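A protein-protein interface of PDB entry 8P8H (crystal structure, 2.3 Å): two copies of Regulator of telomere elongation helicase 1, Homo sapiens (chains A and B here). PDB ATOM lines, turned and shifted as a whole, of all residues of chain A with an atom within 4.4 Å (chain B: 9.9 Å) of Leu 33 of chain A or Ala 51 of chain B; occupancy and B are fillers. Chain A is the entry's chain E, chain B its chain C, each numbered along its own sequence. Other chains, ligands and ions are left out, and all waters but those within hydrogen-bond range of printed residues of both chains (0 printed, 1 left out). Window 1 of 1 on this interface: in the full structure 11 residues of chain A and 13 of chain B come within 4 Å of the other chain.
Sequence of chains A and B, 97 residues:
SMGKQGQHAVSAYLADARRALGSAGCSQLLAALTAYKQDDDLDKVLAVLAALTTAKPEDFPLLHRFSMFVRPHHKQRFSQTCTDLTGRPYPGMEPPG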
ATOM      1  N   VAL A  10      -6.069  -9.205  -0.142  1.00  0.00           N
ATOM      2  CA  VAL A  10      -5.826 -10.624  -0.329  1.00  0.00           C
ATOM      3  C   VAL A  10      -5.283 -11.260   0.946  1.00  0.00           C
ATOM      4  O   VAL A  10      -5.816 -12.272   1.394  1.00  0.00           O
ATOM      5  CB  VAL A  10      -4.835 -10.866  -1.482  1.00  0.00           C
ATOM      6  CG1 VAL A  10      -4.466 -12.319  -1.575  1.00  0.00           C
ATOM      7  CG2 VAL A  10      -5.355 -10.349  -2.813  1.00  0.00           C
ATOM      8  N   LEU A  29     -10.146 -24.577  -0.491  1.00  0.00           N
ATOM      9  CA  LEU A  29     -10.609 -23.370  -1.123  1.00  0.00           C
ATOM     10  C   LEU A  29      -9.553 -22.797  -2.082  1.00  0.00           C
ATOM     11  O   LEU A  29      -9.878 -22.294  -3.161  1.00  0.00           O
ATOM     12  CB  LEU A  29     -10.970 -22.369  -0.047  1.00  0.00           C
ATOM     13  CG  LEU A  29     -11.368 -20.990  -0.567  1.00  0.00           C
ATOM     14  CD1 LEU A  29     -12.525 -21.167  -1.498  1.00  0.00           C
ATOM     15  CD2 LEU A  29     -11.672 -20.011   0.543  1.00  0.00           C
ATOM     16  N   LEU A  30      -8.280 -22.862  -1.692  1.00  0.00           N
ATOM     17  CA  LEU A  30      -7.223 -22.269  -2.513  1.00  0.00           C
ATOM     18  C   LEU A  30      -6.952 -23.142  -3.741  1.00  0.00           C
ATOM     19  O   LEU A  30      -6.641 -22.628  -4.812  1.00  0.00           O
ATOM     20  CB  LEU A  30      -5.952 -22.084  -1.676  1.00  0.00           C
ATOM     21  CG  LEU A  30      -6.039 -20.910  -0.668  1.00  0.00           C
ATOM     22  CD1 LEU A  30      -4.740 -20.734   0.131  1.00  0.00           C
ATOM     23  CD2 LEU A  30      -6.386 -19.569  -1.289  1.00  0.00           C
ATOM     24  N   ALA A  31      -7.018 -24.443  -3.562  1.00  0.00           N
ATOM     25  CA  ALA A  31      -7.019 -25.415  -4.671  1.00  0.00           C
ATOM     26  C   ALA A  31      -8.133 -25.076  -5.682  1.00  0.00           C
ATOM     27  O   ALA A  31      -7.874 -25.041  -6.876  1.00  0.00           O
ATOM     28  CB  ALA A  31      -7.198 -26.855  -4.150  1.00  0.00           C
ATOM     29  N   ALA A  32      -9.328 -24.729  -5.192  1.00  0.00           N
ATOM     30  CA  ALA A  32     -10.428 -24.466  -6.095  1.00  0.00           C
ATOM     31  C   ALA A  32     -10.209 -23.120  -6.790  1.00  0.00           C
ATOM     32  O   ALA A  32     -10.551 -22.943  -7.963  1.00  0.00           O
ATOM     33  CB  ALA A  32     -11.716 -24.502  -5.330  1.00  0.00           C
ATOM     34  N   LEU A  33      -9.609 -22.162  -6.070  1.00  0.00           N
ATOM     35  CA  LEU A  33      -9.236 -20.869  -6.661  1.00  0.00           C
ATOM     36  C   LEU A  33      -8.217 -21.085  -7.786  1.00  0.00           C
ATOM     37  O   LEU A  33      -8.344 -20.529  -8.857  1.00  0.00           O
ATOM     38  CB  LEU A  33      -8.693 -19.925  -5.594  1.00  0.00           C
ATOM     39  CG  LEU A  33      -8.076 -18.626  -6.103  1.00  0.00           C
ATOM     40  CD1 LEU A  33      -9.059 -17.765  -6.885  1.00  0.00           C
ATOM     41  CD2 LEU A  33      -7.525 -17.772  -4.947  1.00  0.00           C
ATOM     42  N   THR A  34      -7.231 -21.937  -7.584  1.00  0.00           N
ATOM     43  CA  THR A  34      -6.226 -22.124  -8.613  1.00  0.00           C
ATOM     44  C   THR A  34      -6.865 -22.795  -9.843  1.00  0.00           C
ATOM     45  O   THR A  34      -6.581 -22.398 -10.983  1.00  0.00           O
ATOM     46  CB  THR A  34      -4.986 -22.831  -8.032  1.00  0.00           C
ATOM     47  OG1 THR A  34      -4.276 -21.861  -7.241  1.00  0.00           O
ATOM     48  CG2 THR A  34      -4.022 -23.372  -9.052  1.00  0.00           C
ATOM     49  N   ALA A  35      -7.712 -23.820  -9.657  1.00  0.00           N
ATOM     50  CA  ALA A  35      -8.467 -24.375 -10.782  1.00  0.00           C
ATOM     51  C   ALA A  35      -9.283 -23.323 -11.545  1.00  0.00           C
ATOM     52  O   ALA A  35      -9.203 -23.230 -12.759  1.00  0.00           O
ATOM     53  CB  ALA A  35      -9.362 -25.499 -10.335  1.00  0.00           C
ATOM     54  N   TYR A  36      -9.970 -22.451 -10.834  1.00  0.00           N
ATOM     55  CA  TYR A  36     -10.705 -21.368 -11.469  1.00  0.00           C
ATOM     56  C   TYR A  36      -9.812 -20.398 -12.257  1.00  0.00           C
ATOM     57  O   TYR A  36     -10.192 -19.925 -13.338  1.00  0.00           O
ATOM     58  CB  TYR A  36     -11.451 -20.567 -10.405  1.00  0.00           C
ATOM     59  CG  TYR A  36     -12.105 -19.299 -10.894  1.00  0.00           C
ATOM     60  CD1 TYR A  36     -13.238 -19.359 -11.695  1.00  0.00           C
ATOM     61  CD2 TYR A  36     -11.627 -18.039 -10.563  1.00  0.00           C
ATOM     62  CE1 TYR A  36     -13.905 -18.205 -12.104  1.00  0.00           C
ATOM     63  CE2 TYR A  36     -12.236 -16.880 -11.020  1.00  0.00           C
ATOM     64  CZ  TYR A  36     -13.391 -16.969 -11.788  1.00  0.00           C
ATOM     65  OH  TYR A  36     -14.043 -15.835 -12.216  1.00  0.00           O
ATOM     66  N   LYS A  37      -8.661 -20.030 -11.685  1.00  0.00           N
ATOM     67  CA  LYS A  37      -7.740 -19.165 -12.385  1.00  0.00           C
ATOM     68  C   LYS A  37      -7.331 -19.797 -13.713  1.00  0.00           C
ATOM     69  O   LYS A  37      -6.908 -19.063 -14.592  1.00  0.00           O
ATOM     70  CB  LYS A  37      -6.450 -18.848 -11.582  1.00  0.00           C
ATOM     71  CG  LYS A  37      -6.621 -17.820 -10.482  1.00  0.00           C
ATOM     72  CD  LYS A  37      -5.481 -17.755  -9.512  1.00  0.00           C
ATOM     73  CE  LYS A  37      -5.743 -16.734  -8.427  1.00  0.00           C
ATOM     74  NZ  LYS A  37      -5.874 -15.392  -9.023  1.00  0.00           N
ATOM     75  N   VAL A  45     -16.045 -23.240  -8.589  1.00  0.00           N
ATOM     76  CA  VAL A  45     -15.292 -22.627  -7.494  1.00  0.00           C
ATOM     77  C   VAL A  45     -16.269 -22.161  -6.408  1.00  0.00           C
ATOM     78  O   VAL A  45     -16.026 -22.343  -5.206  1.00  0.00           O
ATOM     79  CB  VAL A  45     -14.292 -21.545  -7.945  1.00  0.00           C
ATOM     80  CG1 VAL A  45     -14.986 -20.370  -8.588  1.00  0.00           C
ATOM     81  CG2 VAL A  45     -13.454 -21.049  -6.794  1.00  0.00           C
ATOM     82  N   PHE A  66     -15.094 -13.259  -1.052  1.00  0.00           N
ATOM     83  CA  PHE A  66     -14.330 -13.987  -2.051  1.00  0.00           C
ATOM     84  C   PHE A  66     -14.387 -13.275  -3.404  1.00  0.00           C
ATOM     85  O   PHE A  66     -13.592 -13.542  -4.297  1.00  0.00           O
ATOM     86  CB  PHE A  66     -14.776 -15.442  -2.102  1.00  0.00           C
ATOM     87  CG  PHE A  66     -13.933 -16.320  -3.014  1.00  0.00           C
ATOM     88  CD1 PHE A  66     -14.299 -16.487  -4.340  1.00  0.00           C
ATOM     89  CD2 PHE A  66     -12.833 -17.017  -2.558  1.00  0.00           C
ATOM     90  CE1 PHE A  66     -13.530 -17.245  -5.204  1.00  0.00           C
ATOM     91  CE2 PHE A  66     -12.103 -17.822  -3.410  1.00  0.00           C
ATOM     92  CZ  PHE A  66     -12.437 -17.930  -4.733  1.00  0.00           C
ATOM     93  N   PHE A  69     -11.464 -12.246  -5.845  1.00  0.00           N
ATOM     94  CA  PHE A  69     -10.757 -13.174  -6.713  1.00  0.00           C
ATOM     95  C   PHE A  69     -11.542 -13.495  -7.976  1.00  0.00           C
ATOM     96  O   PHE A  69     -11.074 -14.197  -8.866  1.00  0.00           O
ATOM     97  CB  PHE A  69     -10.537 -14.505  -6.000  1.00  0.00           C
ATOM     98  CG  PHE A  69      -9.691 -14.381  -4.771  1.00  0.00           C
ATOM     99  CD1 PHE A  69      -8.335 -14.119  -4.889  1.00  0.00           C
ATOM    100  CD2 PHE A  69     -10.247 -14.527  -3.506  1.00  0.00           C
ATOM    101  CE1 PHE A  69      -7.548 -13.974  -3.762  1.00  0.00           C
ATOM    102  CE2 PHE A  69      -9.467 -14.360  -2.377  1.00  0.00           C
ATOM    103  CZ  PHE A  69      -8.119 -14.052  -2.511  1.00  0.00           C
ATOM    104  N   ALA B  20       6.209  -6.013  -3.014  1.00  0.00           N
ATOM    105  CA  ALA B  20       4.989  -6.207  -3.813  1.00  0.00           C
ATOM    106  C   ALA B  20       3.791  -6.725  -3.008  1.00  0.00           C
ATOM    107  O   ALA B  20       2.690  -6.316  -3.282  1.00  0.00           O
ATOM    108  CB  ALA B  20       5.281  -7.132  -4.968  1.00  0.00           C
ATOM    109  N   LEU B  21       3.943  -7.602  -2.025  1.00  0.00           N
ATOM    110  CA  LEU B  21       2.785  -8.240  -1.393  1.00  0.00           C
ATOM    111  C   LEU B  21       2.462  -7.625  -0.024  1.00  0.00           C
ATOM    112  O   LEU B  21       1.382  -7.844   0.574  1.00  0.00           O
ATOM    113  CB  LEU B  21       3.075  -9.739  -1.223  1.00  0.00           C
ATOM    114  CG  LEU B  21       3.566 -10.471  -2.464  1.00  0.00           C
ATOM    115  CD1 LEU B  21       3.854 -11.924  -2.137  1.00  0.00           C
ATOM    116  CD2 LEU B  21       2.557 -10.384  -3.571  1.00  0.00           C
ATOM    117  N   GLY B  25       1.331 -10.599   3.366  1.00  0.00           N
ATOM    118  CA  GLY B  25       1.409 -11.444   2.192  1.00  0.00           C
ATOM    119  C   GLY B  25       2.742 -12.181   2.113  1.00  0.00           C
ATOM    120  O   GLY B  25       2.805 -13.352   1.725  1.00  0.00           O
ATOM    121  N   GLN B  28       2.703 -14.938   4.535  1.00  0.00           N
ATOM    122  CA  GLN B  28       1.871 -16.066   4.129  1.00  0.00           C
ATOM    123  C   GLN B  28       2.616 -16.927   3.127  1.00  0.00           C
ATOM    124  O   GLN B  28       2.641 -18.140   3.247  1.00  0.00           O
ATOM    125  CB  GLN B  28       0.542 -15.578   3.597  1.00  0.00           C
ATOM    126  CG  GLN B  28      -0.358 -15.119   4.743  1.00  0.00           C
ATOM    127  CD  GLN B  28      -1.421 -14.183   4.243  1.00  0.00           C
ATOM    128  OE1 GLN B  28      -1.388 -13.730   3.094  1.00  0.00           O
ATOM    129  NE2 GLN B  28      -2.421 -13.983   5.079  1.00  0.00           N
ATOM    130  N   LEU B  29       3.322 -16.279   2.226  1.00  0.00           N
ATOM    131  CA  LEU B  29       4.096 -16.972   1.225  1.00  0.00           C
ATOM    132  C   LEU B  29       5.218 -17.779   1.838  1.00  0.00           C
ATOM    133  O   LEU B  29       5.496 -18.917   1.400  1.00  0.00           O
ATOM    134  CB  LEU B  29       4.649 -15.949   0.255  1.00  0.00           C
ATOM    135  CG  LEU B  29       5.447 -16.525  -0.880  1.00  0.00           C
ATOM    136  CD1 LEU B  29       4.632 -17.630  -1.565  1.00  0.00           C
ATOM    137  CD2 LEU B  29       5.694 -15.444  -1.929  1.00  0.00           C
ATOM    138  N   ALA B  32       3.901 -20.756   3.555  1.00  0.00           N
ATOM    139  CA  ALA B  32       3.548 -21.810   2.625  1.00  0.00           C
ATOM    140  C   ALA B  32       4.798 -22.516   2.138  1.00  0.00           C
ATOM    141  O   ALA B  32       4.800 -23.740   1.908  1.00  0.00           O
ATOM    142  CB  ALA B  32       2.760 -21.205   1.508  1.00  0.00           C
ATOM    143  N   ASP B  43       0.950 -28.769  -5.019  1.00  0.00           N
ATOM    144  CA  ASP B  43      -0.292 -28.079  -5.355  1.00  0.00           C
ATOM    145  C   ASP B  43      -0.627 -27.030  -4.274  1.00  0.00           C
ATOM    146  O   ASP B  43      -1.055 -25.915  -4.565  1.00  0.00           O
ATOM    147  CB  ASP B  43      -1.414 -29.080  -5.588  1.00  0.00           C
ATOM    148  CG  ASP B  43      -1.199 -29.962  -6.828  1.00  0.00           C
ATOM    149  OD1 ASP B  43      -0.464 -29.555  -7.782  1.00  0.00           O
ATOM    150  OD2 ASP B  43      -1.749 -31.101  -6.836  1.00  0.00           O
ATOM    151  N   LYS B  44      -0.449 -27.396  -3.008  1.00  0.00           N
ATOM    152  CA  LYS B  44      -0.857 -26.524  -1.937  1.00  0.00           C
ATOM    153  C   LYS B  44       0.031 -25.269  -1.880  1.00  0.00           C
ATOM    154  O   LYS B  44      -0.503 -24.195  -1.703  1.00  0.00           O
ATOM    155  CB  LYS B  44      -0.844 -27.319  -0.644  1.00  0.00           C
ATOM    156  CG  LYS B  44      -1.254 -26.533   0.574  1.00  0.00           C
ATOM    157  CD  LYS B  44      -1.519 -27.493   1.759  1.00  0.00           C
ATOM    158  CE  LYS B  44      -0.190 -27.927   2.262  1.00  0.00           C
ATOM    159  NZ  LYS B  44      -0.285 -29.105   3.125  1.00  0.00           N
ATOM    160  N   VAL B  45       1.334 -25.367  -2.158  1.00  0.00           N
ATOM    161  CA  VAL B  45       2.169 -24.182  -2.083  1.00  0.00           C
ATOM    162  C   VAL B  45       1.897 -23.285  -3.301  1.00  0.00           C
ATOM    163  O   VAL B  45       1.789 -22.074  -3.189  1.00  0.00           O
ATOM    164  CB  VAL B  45       3.667 -24.499  -1.882  1.00  0.00           C
ATOM    165  CG1 VAL B  45       4.256 -25.258  -3.053  1.00  0.00           C
ATOM    166  CG2 VAL B  45       4.470 -23.206  -1.651  1.00  0.00           C
ATOM    167  N   LEU B  46       1.712 -23.879  -4.468  1.00  0.00           N
ATOM    168  CA  LEU B  46       1.383 -23.125  -5.660  1.00  0.00           C
ATOM    169  C   LEU B  46       0.048 -22.385  -5.523  1.00  0.00           C
ATOM    170  O   LEU B  46      -0.138 -21.294  -6.050  1.00  0.00           O
ATOM    171  CB  LEU B  46       1.283 -24.176  -6.770  1.00  0.00           C
ATOM    172  CG  LEU B  46       1.136 -23.747  -8.212  1.00  0.00           C
ATOM    173  CD1 LEU B  46       2.095 -22.622  -8.563  1.00  0.00           C
ATOM    174  CD2 LEU B  46       1.467 -24.943  -9.063  1.00  0.00           C
ATOM    175  N   ALA B  47      -0.912 -22.983  -4.812  1.00  0.00           N
ATOM    176  CA  ALA B  47      -2.209 -22.347  -4.662  1.00  0.00           C
ATOM    177  C   ALA B  47      -2.072 -21.090  -3.808  1.00  0.00           C
ATOM    178  O   ALA B  47      -2.742 -20.094  -4.101  1.00  0.00           O
ATOM    179  CB  ALA B  47      -3.205 -23.328  -4.074  1.00  0.00           C
ATOM    180  N   VAL B  48      -1.255 -21.145  -2.715  1.00  0.00           N
ATOM    181  CA  VAL B  48      -1.016 -19.942  -1.926  1.00  0.00           C
ATOM    182  C   VAL B  48      -0.314 -18.901  -2.800  1.00  0.00           C
ATOM    183  O   VAL B  48      -0.655 -17.725  -2.830  1.00  0.00           O
ATOM    184  CB  VAL B  48      -0.167 -20.193  -0.685  1.00  0.00           C
ATOM    185  CG1 VAL B  48       0.121 -18.871   0.032  1.00  0.00           C
ATOM    186  CG2 VAL B  48      -0.770 -21.166   0.287  1.00  0.00           C
ATOM    187  N   LEU B  49       0.702 -19.347  -3.513  1.00  0.00           N
ATOM    188  CA  LEU B  49       1.485 -18.422  -4.317  1.00  0.00           C
ATOM    189  C   LEU B  49       0.630 -17.777  -5.393  1.00  0.00           C
ATOM    190  O   LEU B  49       0.753 -16.583  -5.642  1.00  0.00           O
ATOM    191  CB  LEU B  49       2.640 -19.230  -4.887  1.00  0.00           C
ATOM    192  CG  LEU B  49       3.527 -18.506  -5.881  1.00  0.00           C
ATOM    193  CD1 LEU B  49       4.457 -17.527  -5.225  1.00  0.00           C
ATOM    194  CD2 LEU B  49       4.354 -19.527  -6.625  1.00  0.00           C
ATOM    195  N   ALA B  50      -0.247 -18.551  -6.049  1.00  0.00           N
ATOM    196  CA  ALA B  50      -1.039 -18.026  -7.148  1.00  0.00           C
ATOM    197  C   ALA B  50      -2.029 -17.008  -6.601  1.00  0.00           C
ATOM    198  O   ALA B  50      -2.271 -15.992  -7.216  1.00  0.00           O
ATOM    199  CB  ALA B  50      -1.749 -19.138  -7.905  1.00  0.00           C
ATOM    200  N   ALA B  51      -2.634 -17.285  -5.453  1.00  0.00           N
ATOM    201  CA  ALA B  51      -3.560 -16.319  -4.869  1.00  0.00           C
ATOM    202  C   ALA B  51      -2.832 -15.000  -4.613  1.00  0.00           C
ATOM    203  O   ALA B  51      -3.357 -13.930  -4.908  1.00  0.00           O
ATOM    204  CB  ALA B  51      -4.168 -16.878  -3.611  1.00  0.00           C
ATOM    205  N   LEU B  52      -1.593 -15.039  -4.095  1.00  0.00           N
ATOM    206  CA  LEU B  52      -0.902 -13.783  -3.730  1.00  0.00           C
ATOM    207  C   LEU B  52      -0.336 -13.038  -4.940  1.00  0.00           C
ATOM    208  O   LEU B  52      -0.375 -11.825  -4.960  1.00  0.00           O
ATOM    209  CB  LEU B  52       0.225 -14.130  -2.758  1.00  0.00           C
ATOM    210  CG  LEU B  52      -0.238 -14.524  -1.370  1.00  0.00           C
ATOM    211  CD1 LEU B  52       0.934 -15.175  -0.675  1.00  0.00           C
ATOM    212  CD2 LEU B  52      -0.818 -13.331  -0.617  1.00  0.00           C
ATOM    213  N   THR B  53       0.203 -13.759  -5.935  1.00  0.00           N
ATOM    214  CA  THR B  53       1.044 -13.147  -6.950  1.00  0.00           C
ATOM    215  C   THR B  53       0.406 -13.116  -8.334  1.00  0.00           C
ATOM    216  O   THR B  53       1.070 -12.691  -9.274  1.00  0.00           O
ATOM    217  CB  THR B  53       2.355 -13.914  -7.126  1.00  0.00           C
ATOM    218  OG1 THR B  53       2.052 -15.188  -7.701  1.00  0.00           O
ATOM    219  CG2 THR B  53       3.116 -14.061  -5.826  1.00  0.00           C
ATOM    220  N   THR B  54      -0.845 -13.574  -8.510  1.00  0.00           N
ATOM    221  CA  THR B  54      -1.484 -13.413  -9.803  1.00  0.00           C
ATOM    222  C   THR B  54      -2.730 -12.564  -9.702  1.00  0.00           C
ATOM    223  O   THR B  54      -3.499 -12.566 -10.637  1.00  0.00           O
ATOM    224  CB  THR B  54      -1.882 -14.739 -10.484  1.00  0.00           C
ATOM    225  OG1 THR B  54      -2.912 -15.448  -9.788  1.00  0.00           O
ATOM    226  CG2 THR B  54      -0.680 -15.647 -10.660  1.00  0.00           C
ATOM    227  N   ALA B  55      -2.905 -11.812  -8.609  1.00  0.00           N
ATOM    228  CA  ALA B  55      -3.991 -10.837  -8.555  1.00  0.00           C
ATOM    229  C   ALA B  55      -3.744  -9.724  -9.573  1.00  0.00           C
ATOM    230  O   ALA B  55      -4.691  -9.223 -10.171  1.00  0.00           O
ATOM    231  CB  ALA B  55      -4.136 -10.277  -7.170  1.00  0.00           C
ATOM    232  N   LYS B  56      -2.472  -9.347  -9.780  1.00  0.00           N
ATOM    233  CA  LYS B  56      -2.125  -8.305 -10.735  1.00  0.00           C
ATOM    234  C   LYS B  56      -1.003  -8.787 -11.637  1.00  0.00           C
ATOM    235  O   LYS B  56      -0.054  -9.391 -11.154  1.00  0.00           O
ATOM    236  CB  LYS B  56      -1.608  -7.050 -10.031  1.00  0.00           C
ATOM    237  CG  LYS B  56      -2.398  -6.609  -8.808  1.00  0.00           C
ATOM    238  CD  LYS B  56      -1.932  -5.379  -8.200  1.00  0.00           C
ATOM    239  CE  LYS B  56      -0.666  -5.596  -7.418  1.00  0.00           C
ATOM    240  NZ  LYS B  56      -0.247  -4.328  -6.774  1.00  0.00           N
ATOM    241  N   ASP B  59       2.843  -8.667 -10.833  1.00  0.00           N
ATOM    242  CA  ASP B  59       3.370  -9.564  -9.812  1.00  0.00           C
ATOM    243  C   ASP B  59       3.616 -10.968 -10.376  1.00  0.00           C
ATOM    244  O   ASP B  59       4.146 -11.817  -9.663  1.00  0.00           O
ATOM    245  CB  ASP B  59       2.484  -9.656  -8.563  1.00  0.00           C
ATOM    246  CG  ASP B  59       2.248  -8.336  -7.826  1.00  0.00           C
ATOM    247  OD1 ASP B  59       3.036  -7.401  -8.013  1.00  0.00           O
ATOM    248  OD2 ASP B  59       1.236  -8.203  -7.100  1.00  0.00           O
ATOM    249  N   PHE B  60       3.303 -11.215 -11.653  1.00  0.00           N
ATOM    250  CA  PHE B  60       3.495 -12.538 -12.232  1.00  0.00           C
ATOM    251  C   PHE B  60       4.947 -12.988 -12.135  1.00  0.00           C
ATOM    252  O   PHE B  60       5.221 -14.170 -11.994  1.00  0.00           O
ATOM    253  CB  PHE B  60       3.078 -12.621 -13.709  1.00  0.00           C
ATOM    254  CG  PHE B  60       1.606 -12.549 -14.039  1.00  0.00           C
ATOM    255  CD1 PHE B  60       0.634 -12.452 -13.055  1.00  0.00           C
ATOM    256  CD2 PHE B  60       1.190 -12.524 -15.361  1.00  0.00           C
ATOM    257  CE1 PHE B  60      -0.717 -12.473 -13.383  1.00  0.00           C
ATOM    258  CE2 PHE B  60      -0.161 -12.465 -15.693  1.00  0.00           C
ATOM    259  CZ  PHE B  60      -1.118 -12.431 -14.697  1.00  0.00           C
ATOM    260  N   LEU B  62       6.944 -12.844  -9.733  1.00  0.00           N
ATOM    261  CA  LEU B  62       7.104 -13.499  -8.445  1.00  0.00           C
ATOM    262  C   LEU B  62       6.610 -14.942  -8.462  1.00  0.00           C
ATOM    263  O   LEU B  62       7.112 -15.749  -7.674  1.00  0.00           O
ATOM    264  CB  LEU B  62       6.348 -12.705  -7.380  1.00  0.00           C
ATOM    265  CG  LEU B  62       6.919 -11.306  -7.112  1.00  0.00           C
ATOM    266  CD1 LEU B  62       6.147 -10.607  -6.019  1.00  0.00           C
ATOM    267  CD2 LEU B  62       8.386 -11.360  -6.737  1.00  0.00           C
ATOM    268  N   LEU B  63       5.595 -15.237  -9.294  1.00  0.00           N
ATOM    269  CA  LEU B  63       5.146 -16.609  -9.457  1.00  0.00           C
ATOM    270  C   LEU B  63       6.268 -17.417 -10.109  1.00  0.00           C
ATOM    271  O   LEU B  63       6.722 -18.440  -9.567  1.00  0.00           O
ATOM    272  CB  LEU B  63       3.837 -16.638 -10.258  1.00  0.00           C
ATOM    273  CG  LEU B  63       3.269 -18.008 -10.655  1.00  0.00           C
ATOM    274  CD1 LEU B  63       2.744 -18.751  -9.464  1.00  0.00           C
ATOM    275  CD2 LEU B  63       2.130 -17.875 -11.643  1.00  0.00           C
ATOM    276  N   THR B  81       2.129 -25.483 -14.788  1.00  0.00           N
ATOM    277  CA  THR B  81       1.057 -24.800 -14.086  1.00  0.00           C
ATOM    278  C   THR B  81       1.234 -23.292 -14.188  1.00  0.00           C
ATOM    279  O   THR B  81       0.285 -22.553 -14.357  1.00  0.00           O
ATOM    280  CB  THR B  81       0.983 -25.284 -12.642  1.00  0.00           C
ATOM    281  OG1 THR B  81       0.756 -26.684 -12.690  1.00  0.00           O
ATOM    282  CG2 THR B  81      -0.165 -24.652 -11.890  1.00  0.00           C
ATOM    283  N   LEU B  85      -1.206 -20.320 -15.808  1.00  0.00           N
ATOM    284  CA  LEU B  85      -1.781 -19.223 -15.051  1.00  0.00           C
ATOM    285  C   LEU B  85      -1.460 -17.866 -15.704  1.00  0.00           C
ATOM    286  O   LEU B  85      -2.223 -16.927 -15.482  1.00  0.00           O
ATOM    287  CB  LEU B  85      -1.304 -19.348 -13.612  1.00  0.00           C
ATOM    288  CG  LEU B  85      -1.940 -20.479 -12.808  1.00  0.00           C
ATOM    289  CD1 LEU B  85      -1.133 -20.859 -11.577  1.00  0.00           C
ATOM    290  CD2 LEU B  85      -3.353 -20.098 -12.385  1.00  0.00           C
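The backbone carbonyl oxygen of Leu 30 of chain A sits at hydrogen-bond distance from the side-chain hydroxyl of Thr 34 of chain A, 3.5 Å away.
O of Ala 50 of chain B is in hydrogen-bond range of OG1 of Thr 54 of chain B (2.7 Å).
Among the printed residues, merely in contact across the chains: Thr 34 of chain A with Ala 47 of chain B, Lys 37 of chain A with Leu 85 of chain B, Leu 30 of chain A with Ala 47 of chain B, Leu 33 of chain A with Ala 51 of chain B, Lys 37 of chain A with Ala 50 of chain B, Thr 34 of chain A with Ala 50 of chain B, Val 10 of chain A with Ala 51 of chain B, Val 10 of chain A with Leu 52 of chain B and Leu 30 of chain A with Val 48 of chain B.
The side-chain hydroxyl (OG1) of Thr 54 of chain B is in hydrogen-bond range of the side-chain amino group (NZ) of Lys 37 of chain A, at 3.1 Å.
No residue of chain B comes within 4 Å of Ala 32 of chain A.
No residue of chain B comes within 4 Å of Ala 35 of chain A.
Of the printed residues of chain B, Val 10 of chain A touches Ala 51 (3.9 Å) and Leu 52 (3.9 Å).
Of the printed residues of chain A, Ala 47 of chain B touches Leu 30 and Thr 34.
Of the printed residues of chain A, Val 48 of chain B touches Leu 30.
Of the printed residues of chain B, Leu 30 of chain A touches Ala 47 and Val 48.
Of the printed residues of chain B, Lys 37 of chain A touches Ala 50 (3.8 Å), Thr 54 (3.1 Å) and Leu 85 (3.4 Å).
The nearest printed residue of chain A that does not touch Ala 51 of chain B is Leu 30 of chain A (4.2 Å).
The nearest printed residue of chain A that does not touch Ala 50 of chain B is Leu 33 of chain A (5.8 Å).
Of the 26 printed residues of chain B, 7 touch a printed residue of chain A.
Printed residues of chain B that touch a printed residue of chain A: Ala 47, Val 48, Ala 50, Ala 51, Leu 52, Thr 54 and Leu 85.
Hydrophobic or aromatic side chains of chain B within 4 Å of the printed part of chain A: Ala 47, Val 48, Ala 50, Ala 51, Leu 52 and Leu 85.
Among the printed residues, 10 pairs touch across the chains.
Among the printed residues, no Asp or Glu carboxylate lies within 4 Å of a Lys or Arg side-chain nitrogen of the other chain.
3 positions are printed for both chains.
Of the 10 pairs that touch across the chains among the printed residues, none has its exchanged pair printed and touching as well.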
